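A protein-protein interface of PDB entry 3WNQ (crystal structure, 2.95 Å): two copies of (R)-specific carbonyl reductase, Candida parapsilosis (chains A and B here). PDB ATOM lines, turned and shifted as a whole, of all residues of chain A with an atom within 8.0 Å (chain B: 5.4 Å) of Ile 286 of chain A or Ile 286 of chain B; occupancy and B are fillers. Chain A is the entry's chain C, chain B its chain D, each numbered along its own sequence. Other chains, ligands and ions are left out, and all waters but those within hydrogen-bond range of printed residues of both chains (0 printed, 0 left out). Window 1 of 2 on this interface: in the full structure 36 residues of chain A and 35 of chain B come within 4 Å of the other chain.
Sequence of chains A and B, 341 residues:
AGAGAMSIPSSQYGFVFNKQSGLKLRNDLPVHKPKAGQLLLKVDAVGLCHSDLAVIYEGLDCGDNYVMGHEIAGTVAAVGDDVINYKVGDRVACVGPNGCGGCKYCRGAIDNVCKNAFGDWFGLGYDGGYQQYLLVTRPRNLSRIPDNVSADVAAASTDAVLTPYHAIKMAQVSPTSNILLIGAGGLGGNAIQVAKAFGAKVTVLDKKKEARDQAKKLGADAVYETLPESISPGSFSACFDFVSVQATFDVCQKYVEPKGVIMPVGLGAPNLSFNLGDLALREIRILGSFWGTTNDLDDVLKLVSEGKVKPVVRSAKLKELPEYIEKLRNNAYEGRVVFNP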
ATOM      1  N   MET A 170     -18.803  -6.485 -31.590  1.00  0.00           N
ATOM      2  CA  MET A 170     -18.940  -6.752 -30.173  1.00  0.00           C
ATOM      3  C   MET A 170     -18.489  -5.542 -29.388  1.00  0.00           C
ATOM      4  O   MET A 170     -19.060  -5.222 -28.352  1.00  0.00           O
ATOM      5  CB  MET A 170     -18.100  -7.969 -29.757  1.00  0.00           C
ATOM      6  CG  MET A 170     -18.288  -8.443 -28.298  1.00  0.00           C
ATOM      7  SD  MET A 170     -17.552 -10.069 -28.039  1.00  0.00           S
ATOM      8  CE  MET A 170     -18.033 -10.566 -26.109  1.00  0.00           C
ATOM      9  N   CYS A 239      -9.188  -1.661 -27.529  1.00  0.00           N
ATOM     10  CA  CYS A 239      -7.909  -2.227 -27.934  1.00  0.00           C
ATOM     11  C   CYS A 239      -8.073  -3.640 -28.398  1.00  0.00           C
ATOM     12  O   CYS A 239      -8.593  -4.475 -27.640  1.00  0.00           O
ATOM     13  CB  CYS A 239      -6.955  -2.239 -26.763  1.00  0.00           C
ATOM     14  SG  CYS A 239      -6.526  -0.597 -26.332  1.00  0.00           S
ATOM     15  N   PHE A 249      -0.873  -7.464 -24.188  1.00  0.00           N
ATOM     16  CA  PHE A 249      -2.050  -7.227 -23.411  1.00  0.00           C
ATOM     17  C   PHE A 249      -1.776  -6.067 -22.448  1.00  0.00           C
ATOM     18  O   PHE A 249      -2.630  -5.229 -22.205  1.00  0.00           O
ATOM     19  CB  PHE A 249      -2.399  -8.452 -22.629  1.00  0.00           C
ATOM     20  CG  PHE A 249      -3.597  -8.263 -21.767  1.00  0.00           C
ATOM     21  CD1 PHE A 249      -3.475  -7.674 -20.513  1.00  0.00           C
ATOM     22  CD2 PHE A 249      -4.875  -8.602 -22.253  1.00  0.00           C
ATOM     23  CE1 PHE A 249      -4.596  -7.419 -19.757  1.00  0.00           C
ATOM     24  CE2 PHE A 249      -6.017  -8.355 -21.510  1.00  0.00           C
ATOM     25  CZ  PHE A 249      -5.883  -7.759 -20.258  1.00  0.00           C
ATOM     26  N   GLN A 253      -4.038  -2.658 -21.680  1.00  0.00           N
ATOM     27  CA  GLN A 253      -4.528  -2.189 -20.393  1.00  0.00           C
ATOM     28  C   GLN A 253      -3.930  -0.855 -19.978  1.00  0.00           C
ATOM     29  O   GLN A 253      -4.472  -0.118 -19.166  1.00  0.00           O
ATOM     30  CB  GLN A 253      -4.236  -3.206 -19.314  1.00  0.00           C
ATOM     31  CG  GLN A 253      -4.745  -2.772 -17.976  1.00  0.00           C
ATOM     32  CD  GLN A 253      -4.708  -3.869 -16.960  1.00  0.00           C
ATOM     33  OE1 GLN A 253      -4.052  -4.895 -17.162  1.00  0.00           O
ATOM     34  NE2 GLN A 253      -5.404  -3.660 -15.841  1.00  0.00           N
ATOM     35  N   GLY A 260     -13.248   1.367 -21.082  1.00  0.00           N
ATOM     36  CA  GLY A 260     -12.864   0.837 -22.382  1.00  0.00           C
ATOM     37  C   GLY A 260     -12.926  -0.682 -22.546  1.00  0.00           C
ATOM     38  O   GLY A 260     -13.307  -1.406 -21.640  1.00  0.00           O
ATOM     39  N   VAL A 261     -12.528  -1.161 -23.713  1.00  0.00           N
ATOM     40  CA  VAL A 261     -12.606  -2.569 -24.046  1.00  0.00           C
ATOM     41  C   VAL A 261     -11.266  -3.092 -24.502  1.00  0.00           C
ATOM     42  O   VAL A 261     -10.635  -2.487 -25.371  1.00  0.00           O
ATOM     43  CB  VAL A 261     -13.596  -2.809 -25.264  1.00  0.00           C
ATOM     44  CG1 VAL A 261     -13.879  -4.306 -25.478  1.00  0.00           C
ATOM     45  CG2 VAL A 261     -14.873  -2.037 -25.054  1.00  0.00           C
ATOM     46  N   ILE A 262     -10.831  -4.215 -23.930  1.00  0.00           N
ATOM     47  CA  ILE A 262      -9.581  -4.857 -24.337  1.00  0.00           C
ATOM     48  C   ILE A 262     -10.033  -6.176 -24.903  1.00  0.00           C
ATOM     49  O   ILE A 262     -10.697  -6.965 -24.229  1.00  0.00           O
ATOM     50  CB  ILE A 262      -8.646  -5.146 -23.162  1.00  0.00           C
ATOM     51  CG1 ILE A 262      -8.192  -3.874 -22.472  1.00  0.00           C
ATOM     52  CG2 ILE A 262      -7.444  -5.778 -23.682  1.00  0.00           C
ATOM     53  CD1 ILE A 262      -7.443  -4.120 -21.246  1.00  0.00           C
ATOM     54  N   MET A 263      -9.698  -6.420 -26.151  1.00  0.00           N
ATOM     55  CA  MET A 263     -10.130  -7.664 -26.769  1.00  0.00           C
ATOM     56  C   MET A 263      -8.977  -8.501 -27.291  1.00  0.00           C
ATOM     57  O   MET A 263      -8.430  -8.249 -28.364  1.00  0.00           O
ATOM     58  CB  MET A 263     -11.135  -7.339 -27.853  1.00  0.00           C
ATOM     59  CG  MET A 263     -12.282  -6.566 -27.280  1.00  0.00           C
ATOM     60  SD  MET A 263     -13.720  -6.973 -28.145  1.00  0.00           S
ATOM     61  CE  MET A 263     -13.575  -8.730 -28.470  1.00  0.00           C
ATOM     62  N   PRO A 264      -8.582  -9.505 -26.491  1.00  0.00           N
ATOM     63  CA  PRO A 264      -7.506 -10.450 -26.744  1.00  0.00           C
ATOM     64  C   PRO A 264      -7.942 -11.408 -27.834  1.00  0.00           C
ATOM     65  O   PRO A 264      -8.464 -12.510 -27.584  1.00  0.00           O
ATOM     66  CB  PRO A 264      -7.347 -11.105 -25.399  1.00  0.00           C
ATOM     67  CG  PRO A 264      -8.790 -11.224 -24.942  1.00  0.00           C
ATOM     68  CD  PRO A 264      -9.300  -9.856 -25.246  1.00  0.00           C
ATOM     69  N   LEU A 272      -3.196 -15.020 -19.751  1.00  0.00           N
ATOM     70  CA  LEU A 272      -2.758 -13.641 -19.756  1.00  0.00           C
ATOM     71  C   LEU A 272      -3.229 -13.164 -18.434  1.00  0.00           C
ATOM     72  O   LEU A 272      -4.222 -13.656 -17.902  1.00  0.00           O
ATOM     73  CB  LEU A 272      -3.422 -12.809 -20.848  1.00  0.00           C
ATOM     74  CG  LEU A 272      -3.025 -13.096 -22.293  1.00  0.00           C
ATOM     75  CD1 LEU A 272      -3.971 -12.390 -23.305  1.00  0.00           C
ATOM     76  CD2 LEU A 272      -1.569 -12.697 -22.444  1.00  0.00           C
ATOM     77  N   SER A 273      -2.501 -12.215 -17.887  1.00  0.00           N
ATOM     78  CA  SER A 273      -2.869 -11.694 -16.609  1.00  0.00           C
ATOM     79  C   SER A 273      -3.150 -10.205 -16.757  1.00  0.00           C
ATOM     80  O   SER A 273      -2.606  -9.531 -17.639  1.00  0.00           O
ATOM     81  CB  SER A 273      -1.732 -11.907 -15.617  1.00  0.00           C
ATOM     82  OG  SER A 273      -1.074 -10.668 -15.397  1.00  0.00           O
ATOM     83  N   PHE A 274      -4.016  -9.698 -15.889  1.00  0.00           N
ATOM     84  CA  PHE A 274      -4.342  -8.302 -15.908  1.00  0.00           C
ATOM     85  C   PHE A 274      -4.121  -7.767 -14.501  1.00  0.00           C
ATOM     86  O   PHE A 274      -4.079  -8.534 -13.552  1.00  0.00           O
ATOM     87  CB  PHE A 274      -5.796  -8.137 -16.391  1.00  0.00           C
ATOM     88  CG  PHE A 274      -6.850  -8.768 -15.495  1.00  0.00           C
ATOM     89  CD1 PHE A 274      -7.342  -8.092 -14.380  1.00  0.00           C
ATOM     90  CD2 PHE A 274      -7.393  -9.998 -15.804  1.00  0.00           C
ATOM     91  CE1 PHE A 274      -8.359  -8.632 -13.588  1.00  0.00           C
ATOM     92  CE2 PHE A 274      -8.411 -10.545 -15.017  1.00  0.00           C
ATOM     93  CZ  PHE A 274      -8.893  -9.852 -13.904  1.00  0.00           C
ATOM     94  N   ASN A 275      -3.946  -6.463 -14.363  1.00  0.00           N
ATOM     95  CA  ASN A 275      -3.778  -5.850 -13.058  1.00  0.00           C
ATOM     96  C   ASN A 275      -5.181  -5.596 -12.449  1.00  0.00           C
ATOM     97  O   ASN A 275      -5.900  -4.695 -12.930  1.00  0.00           O
ATOM     98  CB  ASN A 275      -3.046  -4.536 -13.246  1.00  0.00           C
ATOM     99  CG  ASN A 275      -2.742  -3.840 -11.954  1.00  0.00           C
ATOM    100  OD1 ASN A 275      -3.595  -3.206 -11.320  1.00  0.00           O
ATOM    101  ND2 ASN A 275      -1.499  -3.947 -11.549  1.00  0.00           N
ATOM    102  N   LEU A 276      -5.572  -6.362 -11.414  1.00  0.00           N
ATOM    103  CA  LEU A 276      -6.888  -6.193 -10.777  1.00  0.00           C
ATOM    104  C   LEU A 276      -7.228  -4.761 -10.370  1.00  0.00           C
ATOM    105  O   LEU A 276      -8.296  -4.235 -10.693  1.00  0.00           O
ATOM    106  CB  LEU A 276      -7.016  -7.072  -9.539  1.00  0.00           C
ATOM    107  CG  LEU A 276      -8.427  -6.919  -8.974  1.00  0.00           C
ATOM    108  CD1 LEU A 276      -9.393  -7.771  -9.749  1.00  0.00           C
ATOM    109  CD2 LEU A 276      -8.443  -7.299  -7.521  1.00  0.00           C
ATOM    110  N   LEU A 279      -7.951  -2.569 -13.595  1.00  0.00           N
ATOM    111  CA  LEU A 279      -9.171  -3.023 -14.285  1.00  0.00           C
ATOM    112  C   LEU A 279     -10.459  -2.634 -13.550  1.00  0.00           C
ATOM    113  O   LEU A 279     -11.470  -2.234 -14.175  1.00  0.00           O
ATOM    114  CB  LEU A 279      -9.155  -4.536 -14.473  1.00  0.00           C
ATOM    115  CG  LEU A 279     -10.440  -5.048 -15.147  1.00  0.00           C
ATOM    116  CD1 LEU A 279     -10.122  -6.059 -16.202  1.00  0.00           C
ATOM    117  CD2 LEU A 279     -11.336  -5.674 -14.131  1.00  0.00           C
ATOM    118  N   GLU A 283     -12.969   0.563 -14.488  1.00  0.00           N
ATOM    119  CA  GLU A 283     -14.035  -0.211 -15.082  1.00  0.00           C
ATOM    120  C   GLU A 283     -13.763  -0.807 -16.432  1.00  0.00           C
ATOM    121  O   GLU A 283     -14.698  -0.986 -17.222  1.00  0.00           O
ATOM    122  CB  GLU A 283     -15.317   0.609 -15.102  1.00  0.00           C
ATOM    123  CG  GLU A 283     -15.686   1.103 -13.725  1.00  0.00           C
ATOM    124  CD  GLU A 283     -17.195   1.195 -13.476  1.00  0.00           C
ATOM    125  OE1 GLU A 283     -17.987   1.820 -14.236  1.00  0.00           O
ATOM    126  OE2 GLU A 283     -17.604   0.631 -12.463  1.00  0.00           O
ATOM    127  N   ILE A 284     -12.490  -1.163 -16.660  1.00  0.00           N
ATOM    128  CA  ILE A 284     -12.040  -1.788 -17.914  1.00  0.00           C
ATOM    129  C   ILE A 284     -12.796  -3.118 -18.161  1.00  0.00           C
ATOM    130  O   ILE A 284     -13.029  -3.890 -17.222  1.00  0.00           O
ATOM    131  CB  ILE A 284     -10.521  -2.083 -17.880  1.00  0.00           C
ATOM    132  CG1 ILE A 284      -9.732  -0.933 -18.466  1.00  0.00           C
ATOM    133  CG2 ILE A 284     -10.206  -3.202 -18.792  1.00  0.00           C
ATOM    134  CD1 ILE A 284      -9.888   0.278 -17.717  1.00  0.00           C
ATOM    135  N   ARG A 285     -13.178  -3.385 -19.405  1.00  0.00           N
ATOM    136  CA  ARG A 285     -13.899  -4.579 -19.737  1.00  0.00           C
ATOM    137  C   ARG A 285     -13.040  -5.444 -20.677  1.00  0.00           C
ATOM    138  O   ARG A 285     -12.505  -4.952 -21.664  1.00  0.00           O
ATOM    139  CB  ARG A 285     -15.215  -4.184 -20.422  1.00  0.00           C
ATOM    140  CG  ARG A 285     -15.934  -3.105 -19.699  1.00  0.00           C
ATOM    141  CD  ARG A 285     -17.349  -2.962 -20.191  1.00  0.00           C
ATOM    142  NE  ARG A 285     -17.590  -1.690 -20.893  1.00  0.00           N
ATOM    143  CZ  ARG A 285     -17.331  -1.456 -22.185  1.00  0.00           C
ATOM    144  NH1 ARG A 285     -16.820  -2.414 -22.945  1.00  0.00           N
ATOM    145  NH2 ARG A 285     -17.568  -0.262 -22.724  1.00  0.00           N
ATOM    146  N   ILE A 286     -12.878  -6.727 -20.372  1.00  0.00           N
ATOM    147  CA  ILE A 286     -12.139  -7.630 -21.258  1.00  0.00           C
ATOM    148  C   ILE A 286     -13.190  -8.541 -21.861  1.00  0.00           C
ATOM    149  O   ILE A 286     -13.776  -9.358 -21.157  1.00  0.00           O
ATOM    150  CB  ILE A 286     -11.178  -8.524 -20.474  1.00  0.00           C
ATOM    151  CG1 ILE A 286     -10.048  -7.705 -19.848  1.00  0.00           C
ATOM    152  CG2 ILE A 286     -10.627  -9.573 -21.383  1.00  0.00           C
ATOM    153  CD1 ILE A 286      -9.231  -8.474 -18.825  1.00  0.00           C
ATOM    154  N   LEU A 287     -13.442  -8.416 -23.141  1.00  0.00           N
ATOM    155  CA  LEU A 287     -14.458  -9.241 -23.749  1.00  0.00           C
ATOM    156  C   LEU A 287     -13.863 -10.271 -24.663  1.00  0.00           C
ATOM    157  O   LEU A 287     -13.087  -9.941 -25.527  1.00  0.00           O
ATOM    158  CB  LEU A 287     -15.387  -8.397 -24.583  1.00  0.00           C
ATOM    159  CG  LEU A 287     -15.879  -7.092 -23.993  1.00  0.00           C
ATOM    160  CD1 LEU A 287     -16.551  -6.321 -25.128  1.00  0.00           C
ATOM    161  CD2 LEU A 287     -16.821  -7.371 -22.840  1.00  0.00           C
ATOM    162  N   GLY A 288     -14.247 -11.525 -24.503  1.00  0.00           N
ATOM    163  CA  GLY A 288     -13.716 -12.536 -25.380  1.00  0.00           C
ATOM    164  C   GLY A 288     -14.656 -12.725 -26.545  1.00  0.00           C
ATOM    165  O   GLY A 288     -15.880 -12.715 -26.379  1.00  0.00           O
ATOM    166  N   SER A 289     -14.102 -12.850 -27.739  1.00  0.00           N
ATOM    167  CA  SER A 289     -14.939 -13.091 -28.900  1.00  0.00           C
ATOM    168  C   SER A 289     -14.371 -14.274 -29.684  1.00  0.00           C
ATOM    169  O   SER A 289     -13.191 -14.591 -29.594  1.00  0.00           O
ATOM    170  CB  SER A 289     -15.001 -11.863 -29.777  1.00  0.00           C
ATOM    171  OG  SER A 289     -13.684 -11.442 -29.987  1.00  0.00           O
ATOM    172  N   PHE B 249     -10.774 -16.812  -8.908  1.00  0.00           N
ATOM    173  CA  PHE B 249     -11.033 -16.371 -10.250  1.00  0.00           C
ATOM    174  C   PHE B 249     -11.139 -17.617 -11.141  1.00  0.00           C
ATOM    175  O   PHE B 249     -12.008 -17.698 -12.008  1.00  0.00           O
ATOM    176  CB  PHE B 249      -9.897 -15.482 -10.722  1.00  0.00           C
ATOM    177  CG  PHE B 249     -10.081 -14.987 -12.092  1.00  0.00           C
ATOM    178  CD1 PHE B 249      -9.738 -15.786 -13.184  1.00  0.00           C
ATOM    179  CD2 PHE B 249     -10.730 -13.773 -12.315  1.00  0.00           C
ATOM    180  CE1 PHE B 249     -10.051 -15.400 -14.493  1.00  0.00           C
ATOM    181  CE2 PHE B 249     -11.059 -13.359 -13.631  1.00  0.00           C
ATOM    182  CZ  PHE B 249     -10.719 -14.184 -14.721  1.00  0.00           C
ATOM    183  N   ILE B 262     -17.684 -12.428 -15.430  1.00  0.00           N
ATOM    184  CA  ILE B 262     -16.885 -12.718 -14.241  1.00  0.00           C
ATOM    185  C   ILE B 262     -16.542 -11.348 -13.692  1.00  0.00           C
ATOM    186  O   ILE B 262     -15.949 -10.512 -14.371  1.00  0.00           O
ATOM    187  CB  ILE B 262     -15.572 -13.419 -14.557  1.00  0.00           C
ATOM    188  CG1 ILE B 262     -15.826 -14.776 -15.203  1.00  0.00           C
ATOM    189  CG2 ILE B 262     -14.789 -13.597 -13.302  1.00  0.00           C
ATOM    190  CD1 ILE B 262     -14.544 -15.454 -15.654  1.00  0.00           C
ATOM    191  N   PRO B 264     -14.475  -9.604 -10.807  1.00  0.00           N
ATOM    192  CA  PRO B 264     -13.459  -9.614  -9.762  1.00  0.00           C
ATOM    193  C   PRO B 264     -13.651  -8.400  -8.903  1.00  0.00           C
ATOM    194  O   PRO B 264     -13.070  -7.344  -9.091  1.00  0.00           O
ATOM    195  CB  PRO B 264     -12.169  -9.594 -10.551  1.00  0.00           C
ATOM    196  CG  PRO B 264     -12.517  -8.683 -11.697  1.00  0.00           C
ATOM    197  CD  PRO B 264     -13.906  -9.172 -12.094  1.00  0.00           C
ATOM    198  N   PHE B 274      -6.213 -15.152 -16.665  1.00  0.00           N
ATOM    199  CA  PHE B 274      -7.318 -15.909 -17.193  1.00  0.00           C
ATOM    200  C   PHE B 274      -6.790 -16.758 -18.335  1.00  0.00           C
ATOM    201  O   PHE B 274      -5.739 -16.483 -18.887  1.00  0.00           O
ATOM    202  CB  PHE B 274      -8.431 -14.953 -17.650  1.00  0.00           C
ATOM    203  CG  PHE B 274      -8.057 -14.014 -18.771  1.00  0.00           C
ATOM    204  CD1 PHE B 274      -8.169 -14.418 -20.108  1.00  0.00           C
ATOM    205  CD2 PHE B 274      -7.638 -12.717 -18.499  1.00  0.00           C
ATOM    206  CE1 PHE B 274      -7.866 -13.536 -21.169  1.00  0.00           C
ATOM    207  CE2 PHE B 274      -7.332 -11.833 -19.550  1.00  0.00           C
ATOM    208  CZ  PHE B 274      -7.446 -12.251 -20.888  1.00  0.00           C
ATOM    209  N   LEU B 279     -11.612 -18.023 -22.487  1.00  0.00           N
ATOM    210  CA  LEU B 279     -12.291 -16.719 -22.481  1.00  0.00           C
ATOM    211  C   LEU B 279     -12.779 -16.327 -23.848  1.00  0.00           C
ATOM    212  O   LEU B 279     -13.902 -15.807 -24.007  1.00  0.00           O
ATOM    213  CB  LEU B 279     -11.370 -15.619 -21.956  1.00  0.00           C
ATOM    214  CG  LEU B 279     -12.014 -14.245 -21.940  1.00  0.00           C
ATOM    215  CD1 LEU B 279     -11.750 -13.568 -20.649  1.00  0.00           C
ATOM    216  CD2 LEU B 279     -11.462 -13.448 -23.049  1.00  0.00           C
ATOM    217  N   ILE B 284     -16.530 -15.210 -22.872  1.00  0.00           N
ATOM    218  CA  ILE B 284     -16.571 -14.766 -21.473  1.00  0.00           C
ATOM    219  C   ILE B 284     -16.178 -13.277 -21.366  1.00  0.00           C
ATOM    220  O   ILE B 284     -15.258 -12.831 -22.035  1.00  0.00           O
ATOM    221  CB  ILE B 284     -15.577 -15.572 -20.587  1.00  0.00           C
ATOM    222  CG1 ILE B 284     -16.254 -16.783 -20.008  1.00  0.00           C
ATOM    223  CG2 ILE B 284     -15.152 -14.771 -19.431  1.00  0.00           C
ATOM    224  CD1 ILE B 284     -16.747 -17.654 -21.012  1.00  0.00           C
ATOM    225  N   ARG B 285     -16.872 -12.533 -20.510  1.00  0.00           N
ATOM    226  CA  ARG B 285     -16.607 -11.122 -20.344  1.00  0.00           C
ATOM    227  C   ARG B 285     -16.171 -10.854 -18.915  1.00  0.00           C
ATOM    228  O   ARG B 285     -16.820 -11.295 -17.963  1.00  0.00           O
ATOM    229  CB  ARG B 285     -17.875 -10.321 -20.668  1.00  0.00           C
ATOM    230  CG  ARG B 285     -18.554 -10.725 -21.983  1.00  0.00           C
ATOM    231  CD  ARG B 285     -19.678  -9.786 -22.441  1.00  0.00           C
ATOM    232  NE  ARG B 285     -21.041 -10.336 -22.300  1.00  0.00           N
ATOM    233  CZ  ARG B 285     -21.757 -10.398 -21.158  1.00  0.00           C
ATOM    234  NH1 ARG B 285     -21.257  -9.944 -20.002  1.00  0.00           N
ATOM    235  NH2 ARG B 285     -22.992 -10.906 -21.165  1.00  0.00           N
ATOM    236  N   ILE B 286     -15.062 -10.142 -18.758  1.00  0.00           N
ATOM    237  CA  ILE B 286     -14.560  -9.804 -17.426  1.00  0.00           C
ATOM    238  C   ILE B 286     -14.800  -8.321 -17.296  1.00  0.00           C
ATOM    239  O   ILE B 286     -14.126  -7.549 -17.976  1.00  0.00           O
ATOM    240  CB  ILE B 286     -13.052 -10.033 -17.300  1.00  0.00           C
ATOM    241  CG1 ILE B 286     -12.733 -11.510 -17.370  1.00  0.00           C
ATOM    242  CG2 ILE B 286     -12.580  -9.535 -15.987  1.00  0.00           C
ATOM    243  CD1 ILE B 286     -11.292 -11.745 -17.565  1.00  0.00           C
ATOM    244  N   LEU B 287     -15.743  -7.913 -16.434  1.00  0.00           N
ATOM    245  CA  LEU B 287     -16.049  -6.483 -16.273  1.00  0.00           C
ATOM    246  C   LEU B 287     -15.579  -5.946 -14.964  1.00  0.00           C
ATOM    247  O   LEU B 287     -15.909  -6.494 -13.923  1.00  0.00           O
ATOM    248  CB  LEU B 287     -17.527  -6.248 -16.307  1.00  0.00           C
ATOM    249  CG  LEU B 287     -18.299  -6.946 -17.405  1.00  0.00           C
ATOM    250  CD1 LEU B 287     -19.772  -6.778 -17.072  1.00  0.00           C
ATOM    251  CD2 LEU B 287     -17.971  -6.390 -18.782  1.00  0.00           C
ATOM    252  N   GLY B 288     -14.832  -4.855 -14.995  1.00  0.00           N
ATOM    253  CA  GLY B 288     -14.358  -4.299 -13.747  1.00  0.00           C
ATOM    254  C   GLY B 288     -15.339  -3.267 -13.269  1.00  0.00           C
ATOM    255  O   GLY B 288     -15.850  -2.503 -14.079  1.00  0.00           O
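The backbone carbonyl oxygen (O) of Leu 272 of chain A is in hydrogen-bond range of the backbone NH (N) of Phe 274 of chain B. The backbone carbonyl oxygen (O) of Ile 284 of chain A lies within hydrogen-bond range of the backbone NH (N) of Gly 288 of chain B (3.0 Å). N of Ile 286 of chain A lies within hydrogen-bond range of O of Ile 286 of chain B, at 2.8 Å. N of Gly 288 of chain A is in hydrogen-bond range of O of Ile 284 of chain B, 3.0 Å away.
The backbone carbonyl oxygen of Arg 285 of chain A sits at hydrogen-bond distance from the backbone NH of Ile 262 of chain A, at 2.9 Å. The backbone NH of Leu 287 of chain A sits at hydrogen-bond distance from the backbone carbonyl oxygen of Ile 262 of chain A, at 3.3 Å. O of Leu 279 of chain A lies within hydrogen-bond range of N of Ile 284 of chain A, at 2.9 Å. N of Ile 262 of chain B is in hydrogen-bond range of O of Arg 285 of chain B, 2.9 Å away. The backbone carbonyl oxygen (O) of Ile 262 of chain B is in hydrogen-bond range of the backbone NH (N) of Leu 287 of chain B (3.3 Å). O of Leu 279 of chain B lies within hydrogen-bond range of N of Ile 284 of chain B, at 2.9 Å.
Among the printed residues, pairs that only touch across the chains: Pro 264 of chain A with Leu 279 of chain B (3.96 Å), Phe 274 of chain A with Phe 274 of chain B (3.8 Å), Leu 276 of chain A with Pro 264 of chain B (3.4 Å), Leu 279 of chain A with Gly 288 of chain B (3.3 Å), Glu 283 of chain A with Gly 288 of chain B (3.1 Å), Ile 284 of chain A with Ile 286 of chain B (3.9 Å), Ile 284 of chain A with Leu 287 of chain B (3.98 Å), Arg 285 of chain A with Ile 286 of chain B (3.5 Å), Arg 285 of chain A with Leu 287 of chain B (3.8 Å), Ile 286 of chain A with Phe 274 of chain B (3.9 Å), Ile 286 of chain A with Ile 284 of chain B (3.9 Å), Ile 286 of chain A with Arg 285 of chain B (3.4 Å), Leu 287 of chain A with Ile 284 of chain B (3.9 Å), Leu 287 of chain A with Arg 285 of chain B (3.8 Å) and Gly 288 of chain A with Leu 279 of chain B (3.4 Å).
Ile 286 of chain A touches just these residues of chain B: Phe 274, Ile 284, Arg 285 and Ile 286. Of chain A, only Ile 284, Arg 285 and Ile 286 come within 4 Å of Ile 286 of chain B. Printed residues of chain B within 4 Å of Arg 285 of chain A: Ile 286 (3.5 Å) and Leu 287 (3.8 Å). Of the printed residues of chain B, Leu 276 of chain A touches Pro 264 (3.4 Å). Printed residues of chain B within 4 Å of Leu 287 of chain A: Ile 284 (3.9 Å) and Arg 285 (3.8 Å). Gly 260 of chain A touches none of the printed residues of chain B. Asn 275 of chain A touches none of the printed residues of chain B. The nearest residue of chain B that does not touch Ile 286 of chain A is Leu 279 of chain B (4.2 Å). The nearest residue of chain A that does not touch Ile 286 of chain B is Phe 274 of chain A (4.03 Å).
Of the 10 printed residues of chain B, 8 touch a printed residue of chain A.
Phe 274 of chain B touches its own counterpart, Phe 274 of chain A. Ile 284 of chain A touches Leu 287 of chain B, and with the chains exchanged Leu 287 of chain A touches Ile 284 of chain B. Ile 284 of chain A touches Gly 288 of chain B, and with the chains exchanged Gly 288 of chain A touches Ile 284 of chain B. Ile 286 of chain A touches its own counterpart, Ile 286 of chain B.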
